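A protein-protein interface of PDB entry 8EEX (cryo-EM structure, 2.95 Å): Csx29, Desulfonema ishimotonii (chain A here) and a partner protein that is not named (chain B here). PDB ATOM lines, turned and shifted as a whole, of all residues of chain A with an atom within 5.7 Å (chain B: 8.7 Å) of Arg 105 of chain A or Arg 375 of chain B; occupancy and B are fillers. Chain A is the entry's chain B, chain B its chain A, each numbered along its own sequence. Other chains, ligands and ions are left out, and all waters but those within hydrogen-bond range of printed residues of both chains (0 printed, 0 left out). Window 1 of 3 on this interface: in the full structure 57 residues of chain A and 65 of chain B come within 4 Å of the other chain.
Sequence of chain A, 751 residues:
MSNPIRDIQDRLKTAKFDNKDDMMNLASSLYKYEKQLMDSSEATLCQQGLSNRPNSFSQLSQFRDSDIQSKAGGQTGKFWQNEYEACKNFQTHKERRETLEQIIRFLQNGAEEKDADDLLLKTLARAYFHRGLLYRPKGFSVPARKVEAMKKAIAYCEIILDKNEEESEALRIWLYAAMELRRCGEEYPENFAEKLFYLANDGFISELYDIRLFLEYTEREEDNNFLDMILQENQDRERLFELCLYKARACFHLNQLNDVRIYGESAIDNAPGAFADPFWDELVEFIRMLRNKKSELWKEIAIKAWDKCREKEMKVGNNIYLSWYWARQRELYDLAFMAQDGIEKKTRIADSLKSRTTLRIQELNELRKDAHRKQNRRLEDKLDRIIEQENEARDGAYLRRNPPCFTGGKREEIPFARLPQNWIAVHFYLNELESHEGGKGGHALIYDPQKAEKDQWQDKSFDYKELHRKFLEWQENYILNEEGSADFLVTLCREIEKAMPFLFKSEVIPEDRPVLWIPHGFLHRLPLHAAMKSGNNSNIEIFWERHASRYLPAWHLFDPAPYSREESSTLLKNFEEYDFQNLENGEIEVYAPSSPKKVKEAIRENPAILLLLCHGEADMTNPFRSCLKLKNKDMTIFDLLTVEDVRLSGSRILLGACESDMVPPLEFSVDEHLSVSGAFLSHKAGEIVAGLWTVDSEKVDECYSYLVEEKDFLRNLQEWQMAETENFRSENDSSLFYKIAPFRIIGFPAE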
ATOM      1  N   LEU A 100       5.842  -1.031  22.322  1.00  0.00           N
ATOM      2  CA  LEU A 100       4.484  -0.549  22.564  1.00  0.00           C
ATOM      3  C   LEU A 100       4.424   0.969  22.524  1.00  0.00           C
ATOM      4  O   LEU A 100       3.476   1.547  21.979  1.00  0.00           O
ATOM      5  CB  LEU A 100       3.972  -1.060  23.910  1.00  0.00           C
ATOM      6  CG  LEU A 100       3.668  -2.553  24.015  1.00  0.00           C
ATOM      7  CD1 LEU A 100       3.486  -2.959  25.461  1.00  0.00           C
ATOM      8  CD2 LEU A 100       2.418  -2.892  23.222  1.00  0.00           C
ATOM      9  N   GLU A 101       5.419   1.636  23.106  1.00  0.00           N
ATOM     10  CA  GLU A 101       5.406   3.093  23.110  1.00  0.00           C
ATOM     11  C   GLU A 101       5.577   3.649  21.702  1.00  0.00           C
ATOM     12  O   GLU A 101       4.947   4.650  21.348  1.00  0.00           O
ATOM     13  CB  GLU A 101       6.487   3.620  24.050  1.00  0.00           C
ATOM     14  CG  GLU A 101       6.112   3.475  25.514  1.00  0.00           C
ATOM     15  CD  GLU A 101       7.243   3.826  26.456  1.00  0.00           C
ATOM     16  OE1 GLU A 101       8.343   4.155  25.968  1.00  0.00           O
ATOM     17  OE2 GLU A 101       7.030   3.771  27.685  1.00  0.00           O
ATOM     18  N   GLN A 102       6.415   3.015  20.878  1.00  0.00           N
ATOM     19  CA  GLN A 102       6.533   3.455  19.490  1.00  0.00           C
ATOM     20  C   GLN A 102       5.208   3.303  18.754  1.00  0.00           C
ATOM     21  O   GLN A 102       4.815   4.181  17.978  1.00  0.00           O
ATOM     22  CB  GLN A 102       7.648   2.696  18.770  1.00  0.00           C
ATOM     23  CG  GLN A 102       9.046   3.048  19.268  1.00  0.00           C
ATOM     24  CD  GLN A 102      10.128   2.828  18.224  1.00  0.00           C
ATOM     25  OE1 GLN A 102       9.848   2.462  17.084  1.00  0.00           O
ATOM     26  NE2 GLN A 102      11.370   3.091  18.605  1.00  0.00           N
ATOM     27  N   ILE A 103       4.500   2.195  18.983  1.00  0.00           N
ATOM     28  CA  ILE A 103       3.189   2.015  18.359  1.00  0.00           C
ATOM     29  C   ILE A 103       2.252   3.149  18.759  1.00  0.00           C
ATOM     30  O   ILE A 103       1.491   3.667  17.934  1.00  0.00           O
ATOM     31  CB  ILE A 103       2.602   0.635  18.716  1.00  0.00           C
ATOM     32  CG1 ILE A 103       3.461  -0.482  18.109  1.00  0.00           C
ATOM     33  CG2 ILE A 103       1.160   0.517  18.224  1.00  0.00           C
ATOM     34  CD1 ILE A 103       3.266  -1.839  18.745  1.00  0.00           C
ATOM     35  N   ILE A 104       2.290   3.552  20.031  1.00  0.00           N
ATOM     36  CA  ILE A 104       1.397   4.610  20.499  1.00  0.00           C
ATOM     37  C   ILE A 104       1.749   5.944  19.850  1.00  0.00           C
ATOM     38  O   ILE A 104       0.877   6.644  19.323  1.00  0.00           O
ATOM     39  CB  ILE A 104       1.423   4.703  22.037  1.00  0.00           C
ATOM     40  CG1 ILE A 104       0.902   3.405  22.663  1.00  0.00           C
ATOM     41  CG2 ILE A 104       0.586   5.883  22.521  1.00  0.00           C
ATOM     42  CD1 ILE A 104       1.304   3.195  24.102  1.00  0.00           C
ATOM     43  N   ARG A 105       3.029   6.326  19.877  1.00  0.00           N
ATOM     44  CA  ARG A 105       3.392   7.655  19.388  1.00  0.00           C
ATOM     45  C   ARG A 105       3.368   7.763  17.868  1.00  0.00           C
ATOM     46  O   ARG A 105       3.353   8.885  17.352  1.00  0.00           O
ATOM     47  CB  ARG A 105       4.757   8.090  19.931  1.00  0.00           C
ATOM     48  CG  ARG A 105       5.962   7.264  19.512  1.00  0.00           C
ATOM     49  CD  ARG A 105       7.293   7.944  19.878  1.00  0.00           C
ATOM     50  NE  ARG A 105       7.814   7.570  21.192  1.00  0.00           N
ATOM     51  CZ  ARG A 105       7.398   8.072  22.350  1.00  0.00           C
ATOM     52  NH1 ARG A 105       6.494   9.038  22.408  1.00  0.00           N
ATOM     53  NH2 ARG A 105       7.916   7.604  23.481  1.00  0.00           N
ATOM     54  N   PHE A 106       3.378   6.645  17.140  1.00  0.00           N
ATOM     55  CA  PHE A 106       3.169   6.714  15.696  1.00  0.00           C
ATOM     56  C   PHE A 106       1.691   6.756  15.327  1.00  0.00           C
ATOM     57  O   PHE A 106       1.316   7.433  14.364  1.00  0.00           O
ATOM     58  CB  PHE A 106       3.859   5.541  14.995  1.00  0.00           C
ATOM     59  CG  PHE A 106       5.332   5.742  14.772  1.00  0.00           C
ATOM     60  CD1 PHE A 106       5.773   6.690  13.869  1.00  0.00           C
ATOM     61  CD2 PHE A 106       6.271   4.983  15.440  1.00  0.00           C
ATOM     62  CE1 PHE A 106       7.115   6.885  13.645  1.00  0.00           C
ATOM     63  CE2 PHE A 106       7.619   5.175  15.218  1.00  0.00           C
ATOM     64  CZ  PHE A 106       8.040   6.127  14.319  1.00  0.00           C
ATOM     65  N   LEU A 107       0.837   6.045  16.066  1.00  0.00           N
ATOM     66  CA  LEU A 107      -0.573   5.935  15.703  1.00  0.00           C
ATOM     67  C   LEU A 107      -1.457   6.956  16.405  1.00  0.00           C
ATOM     68  O   LEU A 107      -2.542   7.265  15.902  1.00  0.00           O
ATOM     69  CB  LEU A 107      -1.096   4.533  16.022  1.00  0.00           C
ATOM     70  CG  LEU A 107      -0.474   3.340  15.296  1.00  0.00           C
ATOM     71  CD1 LEU A 107      -1.297   2.104  15.587  1.00  0.00           C
ATOM     72  CD2 LEU A 107      -0.354   3.574  13.799  1.00  0.00           C
ATOM     73  N   GLN A 108      -1.031   7.478  17.560  1.00  0.00           N
ATOM     74  CA  GLN A 108      -1.813   8.500  18.250  1.00  0.00           C
ATOM     75  C   GLN A 108      -2.067   9.698  17.345  1.00  0.00           C
ATOM     76  O   GLN A 108      -3.094  10.374  17.475  1.00  0.00           O
ATOM     77  CB  GLN A 108      -1.077   8.933  19.525  1.00  0.00           C
ATOM     78  CG  GLN A 108      -1.691  10.091  20.314  1.00  0.00           C
ATOM     79  CD  GLN A 108      -3.043   9.755  20.910  1.00  0.00           C
ATOM     80  OE1 GLN A 108      -3.129   9.313  22.056  1.00  0.00           O
ATOM     81  NE2 GLN A 108      -4.103   9.961  20.140  1.00  0.00           N
ATOM     82  N   ASN A 109      -1.141   9.971  16.422  1.00  0.00           N
ATOM     83  CA  ASN A 109      -1.264  11.120  15.533  1.00  0.00           C
ATOM     84  C   ASN A 109      -2.410  10.959  14.539  1.00  0.00           C
ATOM     85  O   ASN A 109      -2.989  11.960  14.102  1.00  0.00           O
ATOM     86  CB  ASN A 109       0.056  11.326  14.788  1.00  0.00           C
ATOM     87  CG  ASN A 109       0.057  12.569  13.927  1.00  0.00           C
ATOM     88  OD1 ASN A 109      -0.524  13.591  14.287  1.00  0.00           O
ATOM     89  ND2 ASN A 109       0.730  12.492  12.780  1.00  0.00           N
ATOM     90  N   GLY B 369       3.745  15.501   8.195  1.00  0.00           N
ATOM     91  CA  GLY B 369       3.164  15.486   9.534  1.00  0.00           C
ATOM     92  C   GLY B 369       3.141  14.107  10.157  1.00  0.00           C
ATOM     93  O   GLY B 369       2.111  13.685  10.697  1.00  0.00           O
ATOM     94  N   LEU B 370       4.259  13.385  10.074  1.00  0.00           N
ATOM     95  CA  LEU B 370       4.240  11.948  10.324  1.00  0.00           C
ATOM     96  C   LEU B 370       3.982  11.623  11.794  1.00  0.00           C
ATOM     97  O   LEU B 370       3.260  10.668  12.098  1.00  0.00           O
ATOM     98  CB  LEU B 370       5.556  11.332   9.839  1.00  0.00           C
ATOM     99  CG  LEU B 370       5.712   9.812   9.677  1.00  0.00           C
ATOM    100  CD1 LEU B 370       6.000   9.115  10.998  1.00  0.00           C
ATOM    101  CD2 LEU B 370       4.495   9.181   9.006  1.00  0.00           C
ATOM    102  N   LYS B 371       4.566  12.389  12.721  1.00  0.00           N
ATOM    103  CA  LYS B 371       4.467  12.103  14.151  1.00  0.00           C
ATOM    104  C   LYS B 371       3.793  13.226  14.923  1.00  0.00           C
ATOM    105  O   LYS B 371       3.794  14.388  14.507  1.00  0.00           O
ATOM    106  CB  LYS B 371       5.830  11.889  14.825  1.00  0.00           C
ATOM    107  CG  LYS B 371       6.640  10.712  14.358  1.00  0.00           C
ATOM    108  CD  LYS B 371       7.754  10.384  15.366  1.00  0.00           C
ATOM    109  CE  LYS B 371       8.716  11.550  15.634  1.00  0.00           C
ATOM    110  NZ  LYS B 371       9.667  11.210  16.725  1.00  0.00           N
ATOM    111  N   ILE B 372       3.227  12.851  16.068  1.00  0.00           N
ATOM    112  CA  ILE B 372       2.978  13.795  17.152  1.00  0.00           C
ATOM    113  C   ILE B 372       4.258  13.936  17.967  1.00  0.00           C
ATOM    114  O   ILE B 372       4.899  12.938  18.322  1.00  0.00           O
ATOM    115  CB  ILE B 372       1.798  13.341  18.030  1.00  0.00           C
ATOM    116  CG1 ILE B 372       1.521  14.378  19.124  1.00  0.00           C
ATOM    117  CG2 ILE B 372       2.052  11.966  18.674  1.00  0.00           C
ATOM    118  CD1 ILE B 372       0.169  14.222  19.793  1.00  0.00           C
ATOM    119  N   THR B 373       4.648  15.181  18.245  1.00  0.00           N
ATOM    120  CA  THR B 373       5.921  15.431  18.911  1.00  0.00           C
ATOM    121  C   THR B 373       5.840  15.246  20.426  1.00  0.00           C
ATOM    122  O   THR B 373       6.839  14.868  21.048  1.00  0.00           O
ATOM    123  CB  THR B 373       6.425  16.833  18.555  1.00  0.00           C
ATOM    124  OG1 THR B 373       7.781  16.988  18.990  1.00  0.00           O
ATOM    125  CG2 THR B 373       5.560  17.919  19.178  1.00  0.00           C
ATOM    126  N   ARG B 374       4.684  15.499  21.036  1.00  0.00           N
ATOM    127  CA  ARG B 374       4.525  15.253  22.462  1.00  0.00           C
ATOM    128  C   ARG B 374       4.580  13.754  22.747  1.00  0.00           C
ATOM    129  O   ARG B 374       4.252  12.927  21.892  1.00  0.00           O
ATOM    130  CB  ARG B 374       3.199  15.821  22.965  1.00  0.00           C
ATOM    131  CG  ARG B 374       3.216  17.292  23.387  1.00  0.00           C
ATOM    132  CD  ARG B 374       3.662  18.237  22.279  1.00  0.00           C
ATOM    133  NE  ARG B 374       3.306  19.620  22.583  1.00  0.00           N
ATOM    134  CZ  ARG B 374       4.011  20.448  23.345  1.00  0.00           C
ATOM    135  NH1 ARG B 374       5.138  20.069  23.929  1.00  0.00           N
ATOM    136  NH2 ARG B 374       3.567  21.687  23.537  1.00  0.00           N
ATOM    137  N   ARG B 375       5.004  13.406  23.960  1.00  0.00           N
ATOM    138  CA  ARG B 375       5.183  12.010  24.340  1.00  0.00           C
ATOM    139  C   ARG B 375       4.019  11.498  25.196  1.00  0.00           C
ATOM    140  O   ARG B 375       3.054  12.209  25.487  1.00  0.00           O
ATOM    141  CB  ARG B 375       6.538  11.831  25.027  1.00  0.00           C
ATOM    142  CG  ARG B 375       7.673  11.997  24.028  1.00  0.00           C
ATOM    143  CD  ARG B 375       9.043  11.661  24.569  1.00  0.00           C
ATOM    144  NE  ARG B 375      10.033  11.791  23.504  1.00  0.00           N
ATOM    145  CZ  ARG B 375      11.163  11.097  23.422  1.00  0.00           C
ATOM    146  NH1 ARG B 375      11.543  10.268  24.381  1.00  0.00           N
ATOM    147  NH2 ARG B 375      11.933  11.244  22.347  1.00  0.00           N
ATOM    148  N   ILE B 376       4.129  10.228  25.589  1.00  0.00           N
ATOM    149  CA  ILE B 376       2.978   9.384  25.900  1.00  0.00           C
ATOM    150  C   ILE B 376       2.486   9.612  27.323  1.00  0.00           C
ATOM    151  O   ILE B 376       3.279   9.750  28.262  1.00  0.00           O
ATOM    152  CB  ILE B 376       3.349   7.909  25.665  1.00  0.00           C
ATOM    153  CG1 ILE B 376       3.569   7.672  24.168  1.00  0.00           C
ATOM    154  CG2 ILE B 376       2.276   6.974  26.226  1.00  0.00           C
ATOM    155  CD1 ILE B 376       4.345   6.442  23.855  1.00  0.00           C
ATOM    156  N   LEU B 377       1.157   9.627  27.471  1.00  0.00           N
ATOM    157  CA  LEU B 377       0.475   9.651  28.770  1.00  0.00           C
ATOM    158  C   LEU B 377       1.038  10.718  29.707  1.00  0.00           C
ATOM    159  O   LEU B 377       1.347  10.460  30.873  1.00  0.00           O
ATOM    160  CB  LEU B 377       0.483   8.269  29.432  1.00  0.00           C
ATOM    161  CG  LEU B 377      -0.479   7.265  28.788  1.00  0.00           C
ATOM    162  CD1 LEU B 377      -0.083   5.833  29.085  1.00  0.00           C
ATOM    163  CD2 LEU B 377      -1.901   7.528  29.279  1.00  0.00           C
ATOM    164  N   GLY B 378       1.189  11.928  29.180  1.00  0.00           N
ATOM    165  CA  GLY B 378       1.334  13.102  30.017  1.00  0.00           C
ATOM    166  C   GLY B 378      -0.016  13.622  30.469  1.00  0.00           C
ATOM    167  O   GLY B 378      -0.301  14.815  30.330  1.00  0.00           O
ATOM    168  N   ASP B 379      -0.859  12.728  31.012  1.00  0.00           N
ATOM    169  CA  ASP B 379      -2.250  13.073  31.279  1.00  0.00           C
ATOM    170  C   ASP B 379      -2.740  12.561  32.632  1.00  0.00           C
ATOM    171  O   ASP B 379      -3.953  12.597  32.881  1.00  0.00           O
ATOM    172  CB  ASP B 379      -3.141  12.510  30.151  1.00  0.00           C
ATOM    173  CG  ASP B 379      -3.462  13.543  29.087  1.00  0.00           C
ATOM    174  OD1 ASP B 379      -3.881  14.663  29.444  1.00  0.00           O
ATOM    175  OD2 ASP B 379      -3.304  13.229  27.887  1.00  0.00           O
ATOM    176  N   ARG B 503      18.730  17.864  18.097  1.00  0.00           N
ATOM    177  CA  ARG B 503      19.342  16.583  18.417  1.00  0.00           C
ATOM    178  C   ARG B 503      20.257  16.177  17.271  1.00  0.00           C
ATOM    179  O   ARG B 503      19.901  16.339  16.101  1.00  0.00           O
ATOM    180  CB  ARG B 503      18.281  15.509  18.649  1.00  0.00           C
ATOM    181  CG  ARG B 503      18.711  14.393  19.572  1.00  0.00           C
ATOM    182  CD  ARG B 503      18.012  13.097  19.249  1.00  0.00           C
ATOM    183  NE  ARG B 503      16.562  13.281  19.195  1.00  0.00           N
ATOM    184  CZ  ARG B 503      15.762  12.865  18.218  1.00  0.00           C
ATOM    185  NH1 ARG B 503      16.201  12.097  17.232  1.00  0.00           N
ATOM    186  NH2 ARG B 503      14.479  13.215  18.239  1.00  0.00           N
ATOM    187  N   THR B 702      19.462   3.217  23.169  1.00  0.00           N
ATOM    188  CA  THR B 702      18.265   4.046  23.213  1.00  0.00           C
ATOM    189  C   THR B 702      18.091   4.775  24.538  1.00  0.00           C
ATOM    190  O   THR B 702      17.437   5.823  24.570  1.00  0.00           O
ATOM    191  CB  THR B 702      17.021   3.194  22.957  1.00  0.00           C
ATOM    192  OG1 THR B 702      16.940   2.159  23.945  1.00  0.00           O
ATOM    193  CG2 THR B 702      17.069   2.574  21.574  1.00  0.00           C
ATOM    194  N   HIS B 703      18.663   4.256  25.623  1.00  0.00           N
ATOM    195  CA  HIS B 703      18.635   4.916  26.928  1.00  0.00           C
ATOM    196  C   HIS B 703      17.217   5.051  27.489  1.00  0.00           C
ATOM    197  O   HIS B 703      16.893   6.045  28.143  1.00  0.00           O
ATOM    198  CB  HIS B 703      19.318   6.284  26.871  1.00  0.00           C
ATOM    199  CG  HIS B 703      20.749   6.220  26.439  1.00  0.00           C
ATOM    200  ND1 HIS B 703      21.719   5.584  27.186  1.00  0.00           N
ATOM    201  CD2 HIS B 703      21.375   6.700  25.339  1.00  0.00           C
ATOM    202  CE1 HIS B 703      22.880   5.680  26.564  1.00  0.00           C
ATOM    203  NE2 HIS B 703      22.699   6.352  25.442  1.00  0.00           N
ATOM    204  N   SER B 704      16.359   4.067  27.230  1.00  0.00           N
ATOM    205  CA  SER B 704      15.050   3.958  27.867  1.00  0.00           C
ATOM    206  C   SER B 704      15.046   2.736  28.777  1.00  0.00           C
ATOM    207  O   SER B 704      15.493   1.657  28.372  1.00  0.00           O
ATOM    208  CB  SER B 704      13.935   3.851  26.828  1.00  0.00           C
ATOM    209  OG  SER B 704      13.858   5.027  26.039  1.00  0.00           O
ATOM    210  N   SER B 716      18.102  10.750  32.406  1.00  0.00           N
ATOM    211  CA  SER B 716      17.281  10.018  31.454  1.00  0.00           C
ATOM    212  C   SER B 716      15.873  10.582  31.495  1.00  0.00           C
ATOM    213  O   SER B 716      15.553  11.452  32.307  1.00  0.00           O
ATOM    214  CB  SER B 716      17.267   8.520  31.766  1.00  0.00           C
ATOM    215  OG  SER B 716      16.366   7.836  30.916  1.00  0.00           O
ATOM    216  N   GLU B 717      15.027  10.083  30.593  1.00  0.00           N
ATOM    217  CA  GLU B 717      13.599  10.372  30.680  1.00  0.00           C
ATOM    218  C   GLU B 717      12.947   9.708  31.886  1.00  0.00           C
ATOM    219  O   GLU B 717      11.784  10.001  32.176  1.00  0.00           O
ATOM    220  CB  GLU B 717      12.855   9.940  29.406  1.00  0.00           C
ATOM    221  CG  GLU B 717      13.525  10.294  28.070  1.00  0.00           C
ATOM    222  CD  GLU B 717      13.178   9.328  26.952  1.00  0.00           C
ATOM    223  OE1 GLU B 717      13.930   9.285  25.953  1.00  0.00           O
ATOM    224  OE2 GLU B 717      12.152   8.624  27.059  1.00  0.00           O
ATOM    225  N   TYR B 718      13.650   8.803  32.568  1.00  0.00           N
ATOM    226  CA  TYR B 718      13.165   8.151  33.776  1.00  0.00           C
ATOM    227  C   TYR B 718      13.779   8.697  35.059  1.00  0.00           C
ATOM    228  O   TYR B 718      13.320   8.323  36.143  1.00  0.00           O
ATOM    229  CB  TYR B 718      13.431   6.646  33.691  1.00  0.00           C
ATOM    230  CG  TYR B 718      12.587   5.949  32.655  1.00  0.00           C
ATOM    231  CD1 TYR B 718      12.944   5.954  31.319  1.00  0.00           C
ATOM    232  CD2 TYR B 718      11.445   5.259  33.025  1.00  0.00           C
ATOM    233  CE1 TYR B 718      12.169   5.315  30.372  1.00  0.00           C
ATOM    234  CE2 TYR B 718      10.666   4.611  32.091  1.00  0.00           C
ATOM    235  CZ  TYR B 718      11.031   4.640  30.763  1.00  0.00           C
ATOM    236  OH  TYR B 718      10.258   3.990  29.825  1.00  0.00           O
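O of Gly 369 of chain B sits at hydrogen-bond distance from ND2 of Asn 109 of chain A (2.8 Å).
The side-chain amide nitrogen (ND2) of Asn 109 of chain A is in hydrogen-bond range of the backbone carbonyl oxygen (O) of Leu 370 of chain B, 3.2 Å away.
N of Tyr 718 of chain B lies close to OG of Ser 716 of chain B, 3.3 Å away.
The side-chain carboxylate of Glu 717 of chain B is in salt-bridge range of the guanidinium group of Arg 375 of chain B (3.0 Å).
Hydrophobic or aromatic side chains of chain B that line the printed part of chain A: Leu 370, Ile 372, Ile 376 and Tyr 718.
Of the 10 printed residues of chain A, 5 touch a printed residue of chain B.
Glu 101 of chain A touches Ile 376 of chain B.
OH of Tyr 718 of chain B touches OE2 of Glu 101 of chain A, 3.9 Å away.
Ile 376 of chain B touches Ile 104 of chain A (CG1 to CG2, 3.8 Å).
Arg 105 of chain A touches Ile 372 of chain B.
NH1 of Arg 105 of chain A touches CG of Arg 375 of chain B, at 3.6 Å.
Arg 105 of chain A touches Ile 376 of chain B (NH1 to CD1, 3.7 Å).
Phe 106 of chain A touches Leu 370 of chain B.
CE1 of Phe 106 of chain A touches CG of Lys 371 of chain B, 3.9 Å away.
Asn 109 of chain A touches Lys 371 of chain B (ND2 to C, 3.8 Å).
Ile 372 of chain B touches Asn 109 of chain A.
Of chain B, only Ile 372, Arg 375 and Ile 376 come within 4 Å of Arg 105 of chain A.
Of the printed residues of chain A, Arg 375 of chain B touches Arg 105.
Printed residues of chain B within 4 Å of Glu 101 of chain A: Ile 376 (3.1 Å) and Tyr 718 (3.9 Å).
Printed residues of chain A within 4 Å of Gly 369 of chain B: Asn 109.
Of the printed residues of chain B, Phe 106 of chain A touches Leu 370 and Lys 371.
Glu 717 of chain B touches none of the printed residues of chain A.
Arg 503 of chain B touches none of the printed residues of chain A.
The nearest printed residue of chain B that does not touch Asn 109 of chain A is Thr 373 of chain B (6.7 Å).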
